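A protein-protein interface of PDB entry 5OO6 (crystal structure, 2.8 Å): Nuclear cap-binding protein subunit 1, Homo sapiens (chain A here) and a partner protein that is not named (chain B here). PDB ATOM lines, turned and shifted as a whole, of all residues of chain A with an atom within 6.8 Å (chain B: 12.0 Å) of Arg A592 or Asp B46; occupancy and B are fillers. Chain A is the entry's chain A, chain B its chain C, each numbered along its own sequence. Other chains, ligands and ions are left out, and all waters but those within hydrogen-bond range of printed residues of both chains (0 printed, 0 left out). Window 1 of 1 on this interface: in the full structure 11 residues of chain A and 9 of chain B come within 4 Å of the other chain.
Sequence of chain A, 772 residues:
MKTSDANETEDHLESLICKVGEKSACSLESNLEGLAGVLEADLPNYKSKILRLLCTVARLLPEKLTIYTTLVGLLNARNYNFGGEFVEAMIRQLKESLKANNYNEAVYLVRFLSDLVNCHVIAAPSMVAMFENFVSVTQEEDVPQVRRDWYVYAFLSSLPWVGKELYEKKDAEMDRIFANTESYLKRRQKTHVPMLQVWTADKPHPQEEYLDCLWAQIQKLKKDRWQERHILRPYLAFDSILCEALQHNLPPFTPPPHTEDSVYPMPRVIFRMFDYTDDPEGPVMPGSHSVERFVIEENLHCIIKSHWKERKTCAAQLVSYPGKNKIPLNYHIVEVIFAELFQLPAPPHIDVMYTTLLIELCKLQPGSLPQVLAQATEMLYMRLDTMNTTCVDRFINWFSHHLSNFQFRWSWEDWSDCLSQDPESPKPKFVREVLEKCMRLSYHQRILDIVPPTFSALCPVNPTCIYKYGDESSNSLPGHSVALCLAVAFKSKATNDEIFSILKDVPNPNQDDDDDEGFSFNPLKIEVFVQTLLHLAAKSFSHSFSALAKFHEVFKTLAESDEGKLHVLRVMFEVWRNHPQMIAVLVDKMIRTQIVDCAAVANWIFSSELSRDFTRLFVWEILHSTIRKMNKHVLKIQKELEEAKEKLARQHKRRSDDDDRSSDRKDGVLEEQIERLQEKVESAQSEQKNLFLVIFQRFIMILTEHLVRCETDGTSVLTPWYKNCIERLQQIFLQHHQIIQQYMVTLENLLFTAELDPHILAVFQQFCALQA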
ATOM      1  N   LEU A 586       9.761 -25.357   2.085  1.00  0.00           N
ATOM      2  CA  LEU A 586       8.622 -25.813   1.276  1.00  0.00           C
ATOM      3  C   LEU A 586       7.322 -25.660   2.060  1.00  0.00           C
ATOM      4  O   LEU A 586       6.365 -25.050   1.571  1.00  0.00           O
ATOM      5  CB  LEU A 586       8.801 -27.266   0.812  1.00  0.00           C
ATOM      6  CG  LEU A 586       9.782 -27.522  -0.347  1.00  0.00           C
ATOM      7  CD1 LEU A 586       9.876 -29.027  -0.617  1.00  0.00           C
ATOM      8  CD2 LEU A 586       9.408 -26.757  -1.615  1.00  0.00           C
ATOM      9  N   VAL A 587       7.312 -26.198   3.283  1.00  0.00           N
ATOM     10  CA  VAL A 587       6.178 -26.063   4.209  1.00  0.00           C
ATOM     11  C   VAL A 587       5.774 -24.593   4.329  1.00  0.00           C
ATOM     12  O   VAL A 587       4.588 -24.273   4.362  1.00  0.00           O
ATOM     13  CB  VAL A 587       6.498 -26.641   5.611  1.00  0.00           C
ATOM     14  CG1 VAL A 587       5.403 -26.301   6.626  1.00  0.00           C
ATOM     15  CG2 VAL A 587       6.681 -28.156   5.551  1.00  0.00           C
ATOM     16  N   ASP A 588       6.769 -23.708   4.381  1.00  0.00           N
ATOM     17  CA  ASP A 588       6.544 -22.268   4.429  1.00  0.00           C
ATOM     18  C   ASP A 588       5.807 -21.760   3.180  1.00  0.00           C
ATOM     19  O   ASP A 588       4.820 -21.028   3.303  1.00  0.00           O
ATOM     20  CB  ASP A 588       7.879 -21.532   4.613  1.00  0.00           C
ATOM     21  CG  ASP A 588       7.696 -20.005   4.775  1.00  0.00           C
ATOM     22  OD1 ASP A 588       7.420 -19.535   5.899  1.00  0.00           O
ATOM     23  OD2 ASP A 588       7.868 -19.286   3.773  1.00  0.00           O
ATOM     24  N   LYS A 589       6.282 -22.150   1.997  1.00  0.00           N
ATOM     25  CA  LYS A 589       5.680 -21.701   0.740  1.00  0.00           C
ATOM     26  C   LYS A 589       4.287 -22.301   0.571  1.00  0.00           C
ATOM     27  O   LYS A 589       3.380 -21.631   0.078  1.00  0.00           O
ATOM     28  CB  LYS A 589       6.559 -22.068  -0.465  1.00  0.00           C
ATOM     29  CG  LYS A 589       6.144 -21.421  -1.796  1.00  0.00           C
ATOM     30  CD  LYS A 589       6.354 -19.908  -1.846  1.00  0.00           C
ATOM     31  CE  LYS A 589       7.834 -19.539  -1.724  1.00  0.00           C
ATOM     32  NZ  LYS A 589       8.176 -18.205  -2.303  1.00  0.00           N
ATOM     33  N   MET A 590       4.126 -23.557   0.983  1.00  0.00           N
ATOM     34  CA  MET A 590       2.833 -24.232   0.894  1.00  0.00           C
ATOM     35  C   MET A 590       1.774 -23.556   1.782  1.00  0.00           C
ATOM     36  O   MET A 590       0.616 -23.450   1.380  1.00  0.00           O
ATOM     37  CB  MET A 590       2.969 -25.734   1.197  1.00  0.00           C
ATOM     38  CG  MET A 590       3.730 -26.492   0.106  1.00  0.00           C
ATOM     39  SD  MET A 590       3.666 -28.296   0.174  1.00  0.00           S
ATOM     40  CE  MET A 590       4.097 -28.657   1.880  1.00  0.00           C
ATOM     41  N   ILE A 591       2.174 -23.070   2.959  1.00  0.00           N
ATOM     42  CA  ILE A 591       1.269 -22.303   3.825  1.00  0.00           C
ATOM     43  C   ILE A 591       0.967 -20.920   3.234  1.00  0.00           C
ATOM     44  O   ILE A 591      -0.175 -20.471   3.262  1.00  0.00           O
ATOM     45  CB  ILE A 591       1.810 -22.190   5.268  1.00  0.00           C
ATOM     46  CG1 ILE A 591       1.808 -23.568   5.931  1.00  0.00           C
ATOM     47  CG2 ILE A 591       0.929 -21.256   6.110  1.00  0.00           C
ATOM     48  CD1 ILE A 591       2.702 -23.684   7.147  1.00  0.00           C
ATOM     49  N   ARG A 592       1.982 -20.261   2.694  1.00  0.00           N
ATOM     50  CA  ARG A 592       1.819 -18.914   2.130  1.00  0.00           C
ATOM     51  C   ARG A 592       0.921 -18.856   0.894  1.00  0.00           C
ATOM     52  O   ARG A 592       0.211 -17.873   0.696  1.00  0.00           O
ATOM     53  CB  ARG A 592       3.192 -18.281   1.829  1.00  0.00           C
ATOM     54  CG  ARG A 592       3.870 -17.749   3.071  1.00  0.00           C
ATOM     55  CD  ARG A 592       5.299 -17.290   2.818  1.00  0.00           C
ATOM     56  NE  ARG A 592       6.067 -17.123   4.054  1.00  0.00           N
ATOM     57  CZ  ARG A 592       5.900 -16.148   4.958  1.00  0.00           C
ATOM     58  NH1 ARG A 592       4.969 -15.200   4.814  1.00  0.00           N
ATOM     59  NH2 ARG A 592       6.685 -16.127   6.037  1.00  0.00           N
ATOM     60  N   THR A 593       0.952 -19.905   0.075  1.00  0.00           N
ATOM     61  CA  THR A 593       0.132 -19.990  -1.138  1.00  0.00           C
ATOM     62  C   THR A 593      -1.137 -20.842  -0.949  1.00  0.00           C
ATOM     63  O   THR A 593      -1.846 -21.138  -1.919  1.00  0.00           O
ATOM     64  CB  THR A 593       0.965 -20.566  -2.293  1.00  0.00           C
ATOM     65  OG1 THR A 593       1.369 -21.907  -1.973  1.00  0.00           O
ATOM     66  CG2 THR A 593       2.201 -19.697  -2.539  1.00  0.00           C
ATOM     67  N   GLN A 594      -1.405 -21.240   0.299  1.00  0.00           N
ATOM     68  CA  GLN A 594      -2.615 -21.969   0.708  1.00  0.00           C
ATOM     69  C   GLN A 594      -2.757 -23.385   0.152  1.00  0.00           C
ATOM     70  O   GLN A 594      -3.864 -23.922   0.140  1.00  0.00           O
ATOM     71  CB  GLN A 594      -3.875 -21.128   0.457  1.00  0.00           C
ATOM     72  CG  GLN A 594      -3.766 -19.757   1.102  1.00  0.00           C
ATOM     73  CD  GLN A 594      -5.079 -19.039   1.215  1.00  0.00           C
ATOM     74  OE1 GLN A 594      -5.507 -18.347   0.292  1.00  0.00           O
ATOM     75  NE2 GLN A 594      -5.720 -19.179   2.366  1.00  0.00           N
ATOM     76  N   ILE A 595      -1.641 -24.005  -0.253  1.00  0.00           N
ATOM     77  CA  ILE A 595      -1.633 -25.436  -0.600  1.00  0.00           C
ATOM     78  C   ILE A 595      -2.090 -26.204   0.638  1.00  0.00           C
ATOM     79  O   ILE A 595      -2.976 -27.044   0.559  1.00  0.00           O
ATOM     80  CB  ILE A 595      -0.235 -25.988  -1.015  1.00  0.00           C
ATOM     81  CG1 ILE A 595       0.437 -25.172  -2.144  1.00  0.00           C
ATOM     82  CG2 ILE A 595      -0.330 -27.473  -1.387  1.00  0.00           C
ATOM     83  CD1 ILE A 595      -0.452 -24.794  -3.296  1.00  0.00           C
ATOM     84  N   VAL A 596      -1.477 -25.889   1.774  1.00  0.00           N
ATOM     85  CA  VAL A 596      -1.909 -26.390   3.084  1.00  0.00           C
ATOM     86  C   VAL A 596      -2.236 -25.221   4.014  1.00  0.00           C
ATOM     87  O   VAL A 596      -2.047 -24.057   3.654  1.00  0.00           O
ATOM     88  CB  VAL A 596      -0.857 -27.344   3.725  1.00  0.00           C
ATOM     89  CG1 VAL A 596      -0.622 -28.551   2.830  1.00  0.00           C
ATOM     90  CG2 VAL A 596       0.464 -26.637   4.010  1.00  0.00           C
ATOM     91  N   SER A 625       7.732 -21.371  12.987  1.00  0.00           N
ATOM     92  CA  SER A 625       7.593 -20.573  11.770  1.00  0.00           C
ATOM     93  C   SER A 625       6.115 -20.517  11.375  1.00  0.00           C
ATOM     94  O   SER A 625       5.572 -19.445  11.082  1.00  0.00           O
ATOM     95  CB  SER A 625       8.448 -21.143  10.635  1.00  0.00           C
ATOM     96  OG  SER A 625       8.314 -20.370   9.452  1.00  0.00           O
ATOM     97  N   LYS A 629       3.621 -17.158  11.162  1.00  0.00           N
ATOM     98  CA  LYS A 629       2.825 -16.767   9.986  1.00  0.00           C
ATOM     99  C   LYS A 629       1.364 -16.511  10.402  1.00  0.00           C
ATOM    100  O   LYS A 629       0.747 -15.519   9.976  1.00  0.00           O
ATOM    101  CB  LYS A 629       2.877 -17.815   8.874  1.00  0.00           C
ATOM    102  CG  LYS A 629       3.981 -17.619   7.837  1.00  0.00           C
ATOM    103  CD  LYS A 629       4.416 -18.923   7.146  1.00  0.00           C
ATOM    104  CE  LYS A 629       5.303 -19.727   8.076  1.00  0.00           C
ATOM    105  NZ  LYS A 629       5.683 -21.103   7.634  1.00  0.00           N
ATOM    106  N   LYS A 632       1.184 -13.238  12.516  1.00  0.00           N
ATOM    107  CA  LYS A 632       1.359 -12.052  11.663  1.00  0.00           C
ATOM    108  C   LYS A 632       0.144 -11.795  10.789  1.00  0.00           C
ATOM    109  O   LYS A 632      -0.230 -10.640  10.564  1.00  0.00           O
ATOM    110  CB  LYS A 632       2.631 -12.163  10.814  1.00  0.00           C
ATOM    111  CG  LYS A 632       3.899 -11.953  11.620  1.00  0.00           C
ATOM    112  CD  LYS A 632       5.144 -12.277  10.804  1.00  0.00           C
ATOM    113  CE  LYS A 632       6.413 -12.120  11.614  1.00  0.00           C
ATOM    114  NZ  LYS A 632       7.548 -12.691  10.837  1.00  0.00           N
ATOM    115  N   LYS A 636      -1.806  -8.250  10.766  1.00  0.00           N
ATOM    116  CA  LYS A 636      -2.039  -7.471   9.547  1.00  0.00           C
ATOM    117  C   LYS A 636      -3.528  -7.110   9.385  1.00  0.00           C
ATOM    118  O   LYS A 636      -3.857  -5.959   9.064  1.00  0.00           O
ATOM    119  CB  LYS A 636      -1.542  -8.224   8.309  1.00  0.00           C
ATOM    120  CG  LYS A 636      -1.636  -7.443   6.998  1.00  0.00           C
ATOM    121  CD  LYS A 636      -1.364  -8.358   5.805  1.00  0.00           C
ATOM    122  CE  LYS A 636      -1.446  -7.604   4.489  1.00  0.00           C
ATOM    123  NZ  LYS A 636      -0.680  -8.290   3.407  1.00  0.00           N
ATOM    124  N   VAL B  45       2.232 -15.060  -5.519  1.00  0.00           N
ATOM    125  CA  VAL B  45       1.461 -14.109  -4.713  1.00  0.00           C
ATOM    126  C   VAL B  45       1.031 -14.747  -3.387  1.00  0.00           C
ATOM    127  O   VAL B  45       0.509 -15.869  -3.365  1.00  0.00           O
ATOM    128  CB  VAL B  45       0.210 -13.592  -5.478  1.00  0.00           C
ATOM    129  CG1 VAL B  45      -0.568 -12.582  -4.636  1.00  0.00           C
ATOM    130  CG2 VAL B  45       0.607 -12.980  -6.818  1.00  0.00           C
ATOM    131  N   ASP B  46       1.245 -14.015  -2.292  1.00  0.00           N
ATOM    132  CA  ASP B  46       0.879 -14.468  -0.932  1.00  0.00           C
ATOM    133  C   ASP B  46      -0.576 -14.190  -0.629  1.00  0.00           C
ATOM    134  O   ASP B  46      -1.008 -13.035  -0.694  1.00  0.00           O
ATOM    135  CB  ASP B  46       1.750 -13.784   0.136  1.00  0.00           C
ATOM    136  CG  ASP B  46       3.221 -13.928  -0.131  1.00  0.00           C
ATOM    137  OD1 ASP B  46       3.673 -15.012  -0.555  1.00  0.00           O
ATOM    138  OD2 ASP B  46       3.967 -12.940   0.056  1.00  0.00           O
ATOM    139  N   PHE B  47      -1.343 -15.237  -0.317  1.00  0.00           N
ATOM    140  CA  PHE B  47      -2.771 -15.104   0.039  1.00  0.00           C
ATOM    141  C   PHE B  47      -3.000 -15.190   1.560  1.00  0.00           C
ATOM    142  O   PHE B  47      -3.908 -14.551   2.081  1.00  0.00           O
ATOM    143  CB  PHE B  47      -3.606 -16.169  -0.657  1.00  0.00           C
ATOM    144  CG  PHE B  47      -3.533 -16.135  -2.161  1.00  0.00           C
ATOM    145  CD1 PHE B  47      -4.041 -15.051  -2.873  1.00  0.00           C
ATOM    146  CD2 PHE B  47      -2.994 -17.209  -2.869  1.00  0.00           C
ATOM    147  CE1 PHE B  47      -3.993 -15.029  -4.264  1.00  0.00           C
ATOM    148  CE2 PHE B  47      -2.960 -17.201  -4.261  1.00  0.00           C
ATOM    149  CZ  PHE B  47      -3.451 -16.103  -4.957  1.00  0.00           C
ATOM    150  N   PHE B  48      -2.174 -15.975   2.257  1.00  0.00           N
ATOM    151  CA  PHE B  48      -2.199 -16.099   3.710  1.00  0.00           C
ATOM    152  C   PHE B  48      -0.921 -15.477   4.280  1.00  0.00           C
ATOM    153  O   PHE B  48      -0.969 -14.597   5.146  1.00  0.00           O
ATOM    154  CB  PHE B  48      -2.307 -17.585   4.081  1.00  0.00           C
ATOM    155  CG  PHE B  48      -2.317 -17.862   5.566  1.00  0.00           C
ATOM    156  CD1 PHE B  48      -3.507 -17.829   6.290  1.00  0.00           C
ATOM    157  CD2 PHE B  48      -1.142 -18.196   6.230  1.00  0.00           C
ATOM    158  CE1 PHE B  48      -3.518 -18.098   7.648  1.00  0.00           C
ATOM    159  CE2 PHE B  48      -1.147 -18.461   7.588  1.00  0.00           C
ATOM    160  CZ  PHE B  48      -2.337 -18.417   8.297  1.00  0.00           C
ATOM    161  OXT PHE B  48       0.197 -15.834   3.889  1.00  0.00           O
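Of the 15 printed residues of chain A, 3 touch a printed residue of chain B.
Printed residues of chain A that touch a printed residue of chain B: Ile A591, Arg A592 and Gln A594.
Among the printed residues, 6 pairs touch across the chains.
O of Arg A592 is in hydrogen-bond range of N of Phe B48 (3.4 Å).
O of Arg A592 sits at hydrogen-bond distance from N of Phe B47, at 3.2 Å.
Among the printed residues, pairs that only touch across the chains: Ile A591 with Phe B48, Arg A592 with Asp B46, Gln A594 with Phe B47 and Gln A594 with Phe B48.
No residue of chain B comes within 4 Å of Asp A588.
No residue of chain B comes within 4 Å of Lys A589.
Ile A591 touches just one residue of chain B: Phe B48 (3.7 Å).
Arg A592 touches just these residues of chain B: Asp B46, Phe B47 and Phe B48.
No residue of chain B comes within 4 Å of Thr A593.
Of chain B, only Phe B47 and Phe B48 come within 4 Å of Gln A594.
Lys A632 touches none of the printed residues of chain B.
Asp B46 touches one residue of chain A.
Printed residues of chain A within 4 Å of Phe B47: Arg A592 and Gln A594.
Of the printed residues of chain A, Phe B48 touches Ile A591 (3.7 Å), Arg A592 (3.4 Å) and Gln A594 (3.96 Å).
The guanidinium group (NE) of Arg A592 is in salt-bridge range of the side-chain carboxylate (OD2) of Asp A588 (2.8 Å).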
